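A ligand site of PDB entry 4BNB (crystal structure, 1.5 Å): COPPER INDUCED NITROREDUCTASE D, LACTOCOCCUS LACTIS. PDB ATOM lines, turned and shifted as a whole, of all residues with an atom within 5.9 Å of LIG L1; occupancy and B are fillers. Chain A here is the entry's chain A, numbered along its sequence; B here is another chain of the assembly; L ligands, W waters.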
ATOM      1  N   ARG A   9     -32.862 -16.536 -24.758  1.00  0.00           N
ATOM      2  CA  ARG A   9     -32.425 -17.186 -23.527  1.00  0.00           C
ATOM      3  C   ARG A   9     -30.912 -17.334 -23.544  1.00  0.00           C
ATOM      4  O   ARG A   9     -30.359 -17.937 -24.466  1.00  0.00           O
ATOM      5  CB  ARG A   9     -33.062 -18.569 -23.368  1.00  0.00           C
ATOM      6  CG  ARG A   9     -32.666 -19.287 -22.068  1.00  0.00           C
ATOM      7  CD  ARG A   9     -32.385 -20.761 -22.292  1.00  0.00           C
ATOM      8  NE  ARG A   9     -31.439 -20.960 -23.390  1.00  0.00           N
ATOM      9  CZ  ARG A   9     -30.116 -20.854 -23.276  1.00  0.00           C
ATOM     10  NH1 ARG A   9     -29.558 -20.572 -22.100  1.00  0.00           N
ATOM     11  NH2 ARG A   9     -29.351 -21.030 -24.337  1.00  0.00           N
ATOM     12  N   ARG A  10     -30.254 -16.792 -22.529  1.00  0.00           N
ATOM     13  CA  ARG A  10     -28.809 -16.905 -22.416  1.00  0.00           C
ATOM     14  C   ARG A  10     -28.403 -17.060 -20.963  1.00  0.00           C
ATOM     15  O   ARG A  10     -29.168 -16.741 -20.051  1.00  0.00           O
ATOM     16  CB  ARG A  10     -28.112 -15.676 -23.012  1.00  0.00           C
ATOM     17  CG  ARG A  10     -28.299 -15.501 -24.511  1.00  0.00           C
ATOM     18  CD  ARG A  10     -27.601 -16.588 -25.332  1.00  0.00           C
ATOM     19  NE  ARG A  10     -26.177 -16.676 -25.016  1.00  0.00           N
ATOM     20  CZ  ARG A  10     -25.248 -15.844 -25.466  1.00  0.00           C
ATOM     21  NH1 ARG A  10     -25.565 -14.844 -26.263  1.00  0.00           N
ATOM     22  NH2 ARG A  10     -23.985 -16.022 -25.107  1.00  0.00           N
ATOM     23  N   THR A  11     -27.190 -17.554 -20.751  1.00  0.00           N
ATOM     24  CA  THR A  11     -26.595 -17.609 -19.430  1.00  0.00           C
ATOM     25  C   THR A  11     -26.183 -16.206 -19.014  1.00  0.00           C
ATOM     26  O   THR A  11     -25.362 -15.567 -19.675  1.00  0.00           O
ATOM     27  CB  THR A  11     -25.384 -18.555 -19.410  1.00  0.00           C
ATOM     28  OG1 THR A  11     -25.832 -19.912 -19.531  1.00  0.00           O
ATOM     29  CG2 THR A  11     -24.580 -18.400 -18.125  1.00  0.00           C
ATOM     30  N   ILE A  12     -26.797 -15.719 -17.945  1.00  0.00           N
ATOM     31  CA  ILE A  12     -26.502 -14.407 -17.393  1.00  0.00           C
ATOM     32  C   ILE A  12     -26.008 -14.574 -15.970  1.00  0.00           C
ATOM     33  O   ILE A  12     -26.755 -15.011 -15.096  1.00  0.00           O
ATOM     34  CB  ILE A  12     -27.759 -13.508 -17.374  1.00  0.00           C
ATOM     35  CG1 ILE A  12     -28.361 -13.384 -18.779  1.00  0.00           C
ATOM     36  CG2 ILE A  12     -27.431 -12.135 -16.791  1.00  0.00           C
ATOM     37  CD1 ILE A  12     -27.475 -12.657 -19.775  1.00  0.00           C
ATOM     38  N   TYR A  13     -24.737 -14.227 -15.741  1.00  0.00           N
ATOM     39  CA  TYR A  13     -24.144 -14.382 -14.416  1.00  0.00           C
ATOM     40  C   TYR A  13     -24.344 -13.136 -13.546  1.00  0.00           C
ATOM     41  O   TYR A  13     -24.455 -13.235 -12.325  1.00  0.00           O
ATOM     42  CB  TYR A  13     -22.660 -14.711 -14.533  1.00  0.00           C
ATOM     43  CG  TYR A  13     -22.396 -16.101 -15.078  1.00  0.00           C
ATOM     44  CD1 TYR A  13     -22.837 -17.222 -14.396  1.00  0.00           C
ATOM     45  CD2 TYR A  13     -21.698 -16.280 -16.268  1.00  0.00           C
ATOM     46  CE1 TYR A  13     -22.604 -18.495 -14.898  1.00  0.00           C
ATOM     47  CE2 TYR A  13     -21.465 -17.553 -16.770  1.00  0.00           C
ATOM     48  CZ  TYR A  13     -21.918 -18.649 -16.075  1.00  0.00           C
ATOM     49  OH  TYR A  13     -21.682 -19.915 -16.565  1.00  0.00           O
ATOM     50  N   PHE A  91     -24.213 -15.308  -7.032  1.00  0.00           N
ATOM     51  CA  PHE A  91     -25.416 -16.116  -7.045  1.00  0.00           C
ATOM     52  C   PHE A  91     -26.413 -15.601  -6.016  1.00  0.00           C
ATOM     53  O   PHE A  91     -27.605 -15.468  -6.294  1.00  0.00           O
ATOM     54  CB  PHE A  91     -25.085 -17.583  -6.749  1.00  0.00           C
ATOM     55  CG  PHE A  91     -24.224 -18.238  -7.794  1.00  0.00           C
ATOM     56  CD1 PHE A  91     -24.430 -17.964  -9.147  1.00  0.00           C
ATOM     57  CD2 PHE A  91     -23.215 -19.118  -7.445  1.00  0.00           C
ATOM     58  CE1 PHE A  91     -23.644 -18.564 -10.116  1.00  0.00           C
ATOM     59  CE2 PHE A  91     -22.427 -19.711  -8.402  1.00  0.00           C
ATOM     60  CZ  PHE A  91     -22.641 -19.434  -9.738  1.00  0.00           C
ATOM     61  N   VAL A 134     -34.894 -25.777 -19.039  1.00  0.00           N
ATOM     62  CA  VAL A 134     -34.720 -24.809 -20.117  1.00  0.00           C
ATOM     63  C   VAL A 134     -36.024 -24.120 -20.491  1.00  0.00           C
ATOM     64  O   VAL A 134     -36.016 -22.964 -20.908  1.00  0.00           O
ATOM     65  CB  VAL A 134     -34.072 -25.409 -21.379  1.00  0.00           C
ATOM     66  CG1 VAL A 134     -32.725 -26.021 -21.029  1.00  0.00           C
ATOM     67  CG2 VAL A 134     -34.984 -26.422 -22.062  1.00  0.00           C
ATOM     68  N   TRP A 137     -36.232 -21.484 -17.924  1.00  0.00           N
ATOM     69  CA  TRP A 137     -35.161 -20.548 -18.234  1.00  0.00           C
ATOM     70  C   TRP A 137     -35.597 -19.610 -19.374  1.00  0.00           C
ATOM     71  O   TRP A 137     -35.462 -18.389 -19.273  1.00  0.00           O
ATOM     72  CB  TRP A 137     -33.941 -21.370 -18.643  1.00  0.00           C
ATOM     73  CG  TRP A 137     -32.624 -20.687 -18.662  1.00  0.00           C
ATOM     74  CD1 TRP A 137     -32.371 -19.348 -18.621  1.00  0.00           C
ATOM     75  CD2 TRP A 137     -31.353 -21.340 -18.738  1.00  0.00           C
ATOM     76  NE1 TRP A 137     -31.002 -19.131 -18.672  1.00  0.00           N
ATOM     77  CE2 TRP A 137     -30.360 -20.334 -18.734  1.00  0.00           C
ATOM     78  CE3 TRP A 137     -30.951 -22.677 -18.804  1.00  0.00           C
ATOM     79  CZ2 TRP A 137     -29.005 -20.627 -18.801  1.00  0.00           C
ATOM     80  CZ3 TRP A 137     -29.609 -22.968 -18.878  1.00  0.00           C
ATOM     81  CH2 TRP A 137     -28.649 -21.955 -18.870  1.00  0.00           C
ATOM     82  N   ASN A 148     -28.887 -18.295 -14.754  1.00  0.00           N
ATOM     83  CA  ASN A 148     -27.821 -19.239 -15.042  1.00  0.00           C
ATOM     84  C   ASN A 148     -28.102 -20.523 -14.269  1.00  0.00           C
ATOM     85  O   ASN A 148     -28.770 -20.497 -13.245  1.00  0.00           O
ATOM     86  CB  ASN A 148     -26.442 -18.647 -14.703  1.00  0.00           C
ATOM     87  CG  ASN A 148     -26.283 -18.320 -13.233  1.00  0.00           C
ATOM     88  OD1 ASN A 148     -25.981 -19.194 -12.418  1.00  0.00           O
ATOM     89  ND2 ASN A 148     -26.467 -17.051 -12.876  1.00  0.00           N
ATOM     90  N   LEU A 149     -27.604 -21.646 -14.790  1.00  0.00           N
ATOM     91  CA  LEU A 149     -27.891 -22.963 -14.232  1.00  0.00           C
ATOM     92  C   LEU A 149     -26.675 -23.529 -13.525  1.00  0.00           C
ATOM     93  O   LEU A 149     -25.601 -23.621 -14.123  1.00  0.00           O
ATOM     94  CB  LEU A 149     -28.343 -23.911 -15.344  1.00  0.00           C
ATOM     95  CG  LEU A 149     -28.731 -25.333 -14.928  1.00  0.00           C
ATOM     96  CD1 LEU A 149     -29.954 -25.330 -14.017  1.00  0.00           C
ATOM     97  CD2 LEU A 149     -28.975 -26.213 -16.156  1.00  0.00           C
ATOM     98  N   GLN A 150     -26.836 -23.904 -12.262  1.00  0.00           N
ATOM     99  CA  GLN A 150     -25.734 -24.412 -11.453  1.00  0.00           C
ATOM    100  C   GLN A 150     -25.977 -25.829 -10.971  1.00  0.00           C
ATOM    101  O   GLN A 150     -27.112 -26.325 -10.975  1.00  0.00           O
ATOM    102  CB  GLN A 150     -25.487 -23.506 -10.251  1.00  0.00           C
ATOM    103  CG  GLN A 150     -25.073 -22.093 -10.617  1.00  0.00           C
ATOM    104  CD  GLN A 150     -23.907 -22.066 -11.575  1.00  0.00           C
ATOM    105  OE1 GLN A 150     -22.959 -22.846 -11.437  1.00  0.00           O
ATOM    106  NE2 GLN A 150     -23.979 -21.190 -12.564  1.00  0.00           N
ATOM    107  N   HIS A 151     -24.911 -26.482 -10.514  1.00  0.00           N
ATOM    108  CA  HIS A 151     -24.984 -27.861 -10.060  1.00  0.00           C
ATOM    109  C   HIS A 151     -24.158 -28.088  -8.804  1.00  0.00           C
ATOM    110  O   HIS A 151     -23.050 -28.621  -8.850  1.00  0.00           O
ATOM    111  CB  HIS A 151     -24.537 -28.803 -11.179  1.00  0.00           C
ATOM    112  CG  HIS A 151     -25.492 -28.805 -12.330  1.00  0.00           C
ATOM    113  ND1 HIS A 151     -25.349 -27.961 -13.415  1.00  0.00           N
ATOM    114  CD2 HIS A 151     -26.614 -29.511 -12.545  1.00  0.00           C
ATOM    115  CE1 HIS A 151     -26.348 -28.167 -14.257  1.00  0.00           C
ATOM    116  NE2 HIS A 151     -27.128 -29.111 -13.753  1.00  0.00           N
ATOM    117  N   ALA A 185     -24.941 -11.131 -21.757  1.00  0.00           N
ATOM    118  CA  ALA A 185     -24.348 -12.444 -21.907  1.00  0.00           C
ATOM    119  C   ALA A 185     -22.997 -12.314 -22.599  1.00  0.00           C
ATOM    120  O   ALA A 185     -22.751 -11.345 -23.327  1.00  0.00           O
ATOM    121  CB  ALA A 185     -25.257 -13.344 -22.723  1.00  0.00           C
ATOM    122  N   LYS A 188     -20.555 -16.365 -27.581  1.00  0.00           N
ATOM    123  CA  LYS A 188     -20.806 -17.796 -27.709  1.00  0.00           C
ATOM    124  C   LYS A 188     -20.599 -18.256 -29.153  1.00  0.00           C
ATOM    125  O   LYS A 188     -21.039 -17.601 -30.088  1.00  0.00           O
ATOM    126  CB  LYS A 188     -22.226 -18.152 -27.260  1.00  0.00           C
ATOM    127  CG  LYS A 188     -22.535 -19.634 -27.343  1.00  0.00           C
ATOM    128  CD  LYS A 188     -23.863 -19.994 -26.682  1.00  0.00           C
ATOM    129  CE  LYS A 188     -25.046 -19.439 -27.451  1.00  0.00           C
ATOM    130  NZ  LYS A 188     -26.317 -20.092 -27.043  1.00  0.00           N
ATOM    131  N   PHE B  35     -29.867 -22.991 -30.973  1.00  0.00           N
ATOM    132  CA  PHE B  35     -30.089 -22.072 -29.866  1.00  0.00           C
ATOM    133  C   PHE B  35     -30.443 -22.782 -28.560  1.00  0.00           C
ATOM    134  O   PHE B  35     -30.905 -22.152 -27.617  1.00  0.00           O
ATOM    135  CB  PHE B  35     -31.165 -21.059 -30.250  1.00  0.00           C
ATOM    136  CG  PHE B  35     -30.770 -20.189 -31.410  1.00  0.00           C
ATOM    137  CD1 PHE B  35     -29.541 -19.561 -31.434  1.00  0.00           C
ATOM    138  CD2 PHE B  35     -31.614 -20.028 -32.493  1.00  0.00           C
ATOM    139  CE1 PHE B  35     -29.168 -18.761 -32.502  1.00  0.00           C
ATOM    140  CE2 PHE B  35     -31.256 -19.240 -33.568  1.00  0.00           C
ATOM    141  CZ  PHE B  35     -30.025 -18.604 -33.580  1.00  0.00           C
ATOM    142  N   SER B  36     -30.214 -24.093 -28.518  1.00  0.00           N
ATOM    143  CA  SER B  36     -30.407 -24.876 -27.297  1.00  0.00           C
ATOM    144  C   SER B  36     -29.131 -24.911 -26.461  1.00  0.00           C
ATOM    145  O   SER B  36     -28.038 -25.111 -26.995  1.00  0.00           O
ATOM    146  CB  SER B  36     -30.833 -26.301 -27.637  1.00  0.00           C
ATOM    147  OG  SER B  36     -32.133 -26.330 -28.188  1.00  0.00           O
ATOM    148  N   PRO B  37     -29.253 -24.727 -25.143  1.00  0.00           N
ATOM    149  CA  PRO B  37     -28.069 -24.765 -24.275  1.00  0.00           C
ATOM    150  C   PRO B  37     -27.596 -26.179 -23.968  1.00  0.00           C
ATOM    151  O   PRO B  37     -28.403 -27.110 -23.919  1.00  0.00           O
ATOM    152  CB  PRO B  37     -28.551 -24.075 -23.007  1.00  0.00           C
ATOM    153  CG  PRO B  37     -29.995 -24.435 -22.949  1.00  0.00           C
ATOM    154  CD  PRO B  37     -30.476 -24.437 -24.371  1.00  0.00           C
ATOM    155  N   THR B  38     -26.296 -26.329 -23.755  1.00  0.00           N
ATOM    156  CA  THR B  38     -25.693 -27.605 -23.377  1.00  0.00           C
ATOM    157  C   THR B  38     -24.551 -27.340 -22.410  1.00  0.00           C
ATOM    158  O   THR B  38     -23.940 -26.270 -22.452  1.00  0.00           O
ATOM    159  CB  THR B  38     -25.118 -28.353 -24.597  1.00  0.00           C
ATOM    160  OG1 THR B  38     -24.242 -27.492 -25.334  1.00  0.00           O
ATOM    161  CG2 THR B  38     -26.225 -28.853 -25.517  1.00  0.00           C
ATOM    162  N   ALA B  39     -24.265 -28.316 -21.553  1.00  0.00           N
ATOM    163  CA  ALA B  39     -23.162 -28.175 -20.610  1.00  0.00           C
ATOM    164  C   ALA B  39     -21.869 -27.834 -21.344  1.00  0.00           C
ATOM    165  O   ALA B  39     -21.536 -28.457 -22.348  1.00  0.00           O
ATOM    166  CB  ALA B  39     -23.001 -29.455 -19.804  1.00  0.00           C
ATOM    167  N   PHE B  40     -21.161 -26.828 -20.839  1.00  0.00           N
ATOM    168  CA  PHE B  40     -19.896 -26.379 -21.423  1.00  0.00           C
ATOM    169  C   PHE B  40     -20.013 -25.985 -22.897  1.00  0.00           C
ATOM    170  O   PHE B  40     -19.007 -25.963 -23.620  1.00  0.00           O
ATOM    171  CB  PHE B  40     -18.819 -27.449 -21.259  1.00  0.00           C
ATOM    172  CG  PHE B  40     -18.314 -27.589 -19.846  1.00  0.00           C
ATOM    173  CD1 PHE B  40     -17.243 -26.831 -19.413  1.00  0.00           C
ATOM    174  CD2 PHE B  40     -18.921 -28.457 -18.962  1.00  0.00           C
ATOM    175  CE1 PHE B  40     -16.775 -26.949 -18.117  1.00  0.00           C
ATOM    176  CE2 PHE B  40     -18.461 -28.581 -17.669  1.00  0.00           C
ATOM    177  CZ  PHE B  40     -17.385 -27.824 -17.244  1.00  0.00           C
ATOM    178  N   ASN B  41     -21.223 -25.649 -23.333  1.00  0.00           N
ATOM    179  CA  ASN B  41     -21.478 -25.384 -24.746  1.00  0.00           C
ATOM    180  C   ASN B  41     -20.941 -26.514 -25.613  1.00  0.00           C
ATOM    181  O   ASN B  41     -20.424 -26.284 -26.704  1.00  0.00           O
ATOM    182  CB  ASN B  41     -20.838 -24.054 -25.171  1.00  0.00           C
ATOM    183  CG  ASN B  41     -21.373 -23.549 -26.500  1.00  0.00           C
ATOM    184  OD1 ASN B  41     -22.541 -23.771 -26.833  1.00  0.00           O
ATOM    185  ND2 ASN B  41     -20.528 -22.857 -27.260  1.00  0.00           N
ATOM    186  N   TRP B 124     -25.637 -34.811 -18.139  1.00  0.00           N
ATOM    187  CA  TRP B 124     -25.891 -33.534 -18.811  1.00  0.00           C
ATOM    188  C   TRP B 124     -26.141 -33.736 -20.304  1.00  0.00           C
ATOM    189  O   TRP B 124     -26.867 -32.950 -20.932  1.00  0.00           O
ATOM    190  CB  TRP B 124     -24.724 -32.569 -18.590  1.00  0.00           C
ATOM    191  CG  TRP B 124     -24.568 -32.150 -17.160  1.00  0.00           C
ATOM    192  CD1 TRP B 124     -25.566 -32.002 -16.232  1.00  0.00           C
ATOM    193  CD2 TRP B 124     -23.346 -31.839 -16.480  1.00  0.00           C
ATOM    194  NE1 TRP B 124     -25.037 -31.612 -15.032  1.00  0.00           N
ATOM    195  CE2 TRP B 124     -23.673 -31.507 -15.149  1.00  0.00           C
ATOM    196  CE3 TRP B 124     -22.001 -31.804 -16.871  1.00  0.00           C
ATOM    197  CZ2 TRP B 124     -22.709 -31.137 -14.215  1.00  0.00           C
ATOM    198  CZ3 TRP B 124     -21.052 -31.447 -15.943  1.00  0.00           C
ATOM    199  CH2 TRP B 124     -21.406 -31.124 -14.625  1.00  0.00           C
ATOM    200  N   GLN B 127     -29.738 -34.878 -20.561  1.00  0.00           N
ATOM    201  CA  GLN B 127     -30.534 -33.675 -20.387  1.00  0.00           C
ATOM    202  C   GLN B 127     -30.533 -32.867 -21.682  1.00  0.00           C
ATOM    203  O   GLN B 127     -31.576 -32.399 -22.130  1.00  0.00           O
ATOM    204  CB  GLN B 127     -30.023 -32.856 -19.199  1.00  0.00           C
ATOM    205  CG  GLN B 127     -30.264 -33.557 -17.857  1.00  0.00           C
ATOM    206  CD  GLN B 127     -29.647 -32.838 -16.664  1.00  0.00           C
ATOM    207  OE1 GLN B 127     -29.011 -31.800 -16.802  1.00  0.00           O
ATOM    208  NE2 GLN B 127     -29.842 -33.399 -15.481  1.00  0.00           N
ATOM    209  N   GLY B 128     -29.357 -32.757 -22.304  1.00  0.00           N
ATOM    210  CA  GLY B 128     -29.217 -32.068 -23.572  1.00  0.00           C
ATOM    211  C   GLY B 128     -30.070 -32.657 -24.674  1.00  0.00           C
ATOM    212  O   GLY B 128     -30.620 -31.917 -25.509  1.00  0.00           O
ATOM    213  N   ILE B 131     -33.589 -31.612 -24.089  1.00  0.00           N
ATOM    214  CA  ILE B 131     -33.676 -30.187 -24.407  1.00  0.00           C
ATOM    215  C   ILE B 131     -33.862 -29.947 -25.905  1.00  0.00           C
ATOM    216  O   ILE B 131     -34.795 -29.251 -26.309  1.00  0.00           O
ATOM    217  CB  ILE B 131     -32.412 -29.460 -23.888  1.00  0.00           C
ATOM    218  CG1 ILE B 131     -32.455 -29.380 -22.361  1.00  0.00           C
ATOM    219  CG2 ILE B 131     -32.304 -28.061 -24.498  1.00  0.00           C
ATOM    220  CD1 ILE B 131     -31.140 -28.995 -21.722  1.00  0.00           C
HETATM  221  N1  LIG L   1     -23.491 -23.114 -16.522  1.00  0.00           N
HETATM  222  C1  LIG L   1     -22.795 -22.886 -15.216  1.00  0.00           C
HETATM  223  O1  LIG L   1     -22.338 -21.819 -14.973  1.00  0.00           O
HETATM  224  N2  LIG L   1     -22.684 -23.960 -14.265  1.00  0.00           N
HETATM  225  C2  LIG L   1     -23.202 -25.204 -14.535  1.00  0.00           C
HETATM  226  O2  LIG L   1     -23.169 -26.062 -13.720  1.00  0.00           O
HETATM  227  C3  LIG L   1     -23.889 -25.425 -15.814  1.00  0.00           C
HETATM  228  N3  LIG L   1     -24.359 -26.571 -16.098  1.00  0.00           N
HETATM  229  C4  LIG L   1     -25.236 -26.737 -17.317  1.00  0.00           C
HETATM  230  C5  LIG L   1     -25.968 -28.044 -17.532  1.00  0.00           C
HETATM  231  C6  LIG L   1     -26.746 -28.219 -18.580  1.00  0.00           C
HETATM  232  C7  LIG L   1     -27.468 -29.543 -18.788  1.00  0.00           C
HETATM  233  C8  LIG L   1     -26.914 -27.073 -19.598  1.00  0.00           C
HETATM  234  C9  LIG L   1     -27.859 -27.274 -20.779  1.00  0.00           C
HETATM  235  C10 LIG L   1     -26.277 -25.929 -19.419  1.00  0.00           C
HETATM  236  C11 LIG L   1     -25.367 -25.735 -18.209  1.00  0.00           C
HETATM  237  N4  LIG L   1     -24.655 -24.496 -18.006  1.00  0.00           N
HETATM  238  C12 LIG L   1     -23.999 -24.302 -16.796  1.00  0.00           C
HETATM  239  C13 LIG L   1     -24.780 -23.405 -18.956  1.00  0.00           C
HETATM  240  C14 LIG L   1     -24.052 -23.733 -20.254  1.00  0.00           C
HETATM  241  O3  LIG L   1     -22.666 -23.635 -20.081  1.00  0.00           O
HETATM  242  C15 LIG L   1     -24.542 -22.751 -21.315  1.00  0.00           C
HETATM  243  O4  LIG L   1     -25.905 -23.020 -21.505  1.00  0.00           O
HETATM  244  C16 LIG L   1     -23.790 -22.912 -22.639  1.00  0.00           C
HETATM  245  O5  LIG L   1     -22.458 -22.475 -22.506  1.00  0.00           O
HETATM  246  C17 LIG L   1     -24.484 -22.088 -23.716  1.00  0.00           C
HETATM  247  O6  LIG L   1     -24.525 -20.736 -23.342  1.00  0.00           O
HETATM  248  P1  LIG L   1     -25.952 -19.933 -23.181  1.00  0.00           P
HETATM  249  O7  LIG L   1     -26.737 -20.109 -24.405  1.00  0.00           O
HETATM  250  O8  LIG L   1     -26.788 -20.574 -21.918  1.00  0.00           O
HETATM  251  O9  LIG L   1     -25.610 -18.352 -22.912  1.00  0.00           O
HETATM  252  O1  LG2 L   2     -17.948 -22.577 -14.729  1.00  0.00           O
HETATM  253  N1  LG2 L   2     -18.307 -23.817 -14.673  1.00  0.00           N
HETATM  254  O2  LG2 L   2     -17.872 -24.510 -13.781  1.00  0.00           O
HETATM  255  C1  LG2 L   2     -19.207 -24.333 -15.673  1.00  0.00           C
HETATM  256  C2  LG2 L   2     -19.422 -23.539 -16.807  1.00  0.00           C
HETATM  257  C3  LG2 L   2     -20.281 -23.969 -17.812  1.00  0.00           C
HETATM  258  N2  LG2 L   2     -20.908 -25.148 -17.715  1.00  0.00           N
HETATM  259  O3  LG2 L   2     -21.710 -25.528 -18.662  1.00  0.00           O
HETATM  260  C4  LG2 L   2     -20.730 -25.959 -16.621  1.00  0.00           C
HETATM  261  C5  LG2 L   2     -19.901 -25.602 -15.598  1.00  0.00           C
HETATM  262  C6  LG2 L   2     -19.763 -26.505 -14.488  1.00  0.00           C
HETATM  263  C7  LG2 L   2     -20.457 -27.712 -14.469  1.00  0.00           C
HETATM  264  C8  LG2 L   2     -21.298 -28.055 -15.524  1.00  0.00           C
HETATM  265  C9  LG2 L   2     -21.441 -27.192 -16.607  1.00  0.00           C
HETATM  266  O1  LG3 L   3     -20.466 -14.051 -10.887  1.00  0.00           O
HETATM  267  N1  LG3 L   3     -20.485 -15.325 -11.135  1.00  0.00           N
HETATM  268  O2  LG3 L   3     -21.084 -16.057 -10.372  1.00  0.00           O
HETATM  269  C1  LG3 L   3     -19.809 -15.801 -12.310  1.00  0.00           C
HETATM  270  C2  LG3 L   3     -19.242 -14.845 -13.173  1.00  0.00           C
HETATM  271  C3  LG3 L   3     -18.564 -15.234 -14.327  1.00  0.00           C
HETATM  272  N2  LG3 L   3     -18.458 -16.529 -14.641  1.00  0.00           N
HETATM  273  O3  LG3 L   3     -17.823 -16.869 -15.723  1.00  0.00           O
HETATM  274  C4  LG3 L   3     -18.988 -17.503 -13.836  1.00  0.00           C
HETATM  275  C5  LG3 L   3     -19.665 -17.201 -12.678  1.00  0.00           C
HETATM  276  C6  LG3 L   3     -20.194 -18.277 -11.901  1.00  0.00           C
HETATM  277  C7  LG3 L   3     -20.019 -19.598 -12.300  1.00  0.00           C
HETATM  278  C8  LG3 L   3     -19.338 -19.895 -13.479  1.00  0.00           C
HETATM  279  C9  LG3 L   3     -18.821 -18.859 -14.245  1.00  0.00           C
HETATM  280  O   HOH W   1     -21.820 -20.910 -19.212  1.00  0.00           O
HETATM  281  O   HOH W   2     -25.683 -21.190 -16.858  1.00  0.00           O
HETATM  282  O   HOH W   3     -23.128 -17.830 -23.089  1.00  0.00           O
HETATM  283  O   HOH W   4     -21.449 -19.885 -22.986  1.00  0.00           O
HETATM  284  O   HOH W   5     -22.224 -25.530 -10.788  1.00  0.00           O
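Merely in contact with LIG L1: Trp 137, Pro 37 of chain B, Thr 38 of chain B, Ala 39 of chain B, Phe 40 of chain B, Asn 41 of chain B, Gln 127 of chain B and Ile 131 of chain B.
Hydrophobic or aromatic side chains that line LIG L1: Tyr 13, Trp 137, Leu 149, His 151, Pro 37 of chain B, Ala 39 of chain B and Ile 131 of chain B.
16 residues have an atom within 4 Å of LIG L1: Arg 9, Arg 10, Thr 11, Tyr 13, Trp 137, Leu 149, Gln 150, His 151, Lys 188, Pro 37 of chain B, Thr 38 of chain B, Ala 39 of chain B, Phe 40 of chain B, Asn 41 of chain B, Gln 127 of chain B and Ile 131 of chain B.
The nearest printed residue that does not touch LIG L1 is Trp 124 of chain B (4.02 Å).
NE2 of Gln 150 sits at hydrogen-bond distance from OD1 of Asn 148 (2.8 Å).
O of Arg 10 sits at hydrogen-bond distance from NE1 of Trp 137 (3.3 Å).
The side-chain amino group of Lys 188 is in salt-bridge range of an oxygen (O7) of LIG L1, 2.7 Å away.
The backbone NH (N) of Phe 40 of chain B is in hydrogen-bond range of an oxygen (O3) of LG2 L2 (2.6 Å).
An oxygen (O1) of LIG L1 lies within hydrogen-bond range of the side-chain amide nitrogen of Gln 150, 3.0 Å away.
OG1 of Thr 11 sits at hydrogen-bond distance from O8 of LIG L1 (2.7 Å).
The guanidinium group (NE) of Arg 10 is in salt-bridge range of an oxygen (O9) of LIG L1.
The side-chain hydroxyl of Tyr 13 is in hydrogen-bond range of an oxygen (O1) of LIG L1.
The guanidinium group (NH2) of Arg 9 is in salt-bridge range of an oxygen (O7) of LIG L1 (2.8 Å).
ND1 of His 151 lies within hydrogen-bond range of O2 of LIG L1, 2.9 Å away.
The backbone carbonyl oxygen (O) of Leu 149 sits close to a nitrogen (N2) of LIG L1 (2.9 Å).
The backbone NH (N) of Thr 11 lies within hydrogen-bond range of an oxygen (O9) of LIG L1 (2.8 Å).
An oxygen (O3) of LG2 L2 lies within hydrogen-bond range of an oxygen (O3) of LIG L1, 2.6 Å away.
Water W3 lies within hydrogen-bond range of an oxygen (O9) of LIG L1 (2.5 Å) and the guanidinium group (NH2) of Arg 10 (2.8 Å).
Water W2 lies within hydrogen-bond range of the backbone NH of Leu 149, a nitrogen (N1) of LIG L1 and the side-chain hydroxyl of Thr 11.
Water W1 bridges OH of Tyr 13 and O3 of LIG L1.
Water W5 lies within hydrogen-bond range of OE1 of Gln 150 (2.9 Å), N of His 151 (2.9 Å) and O2 of LIG L1 (3.1 Å).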
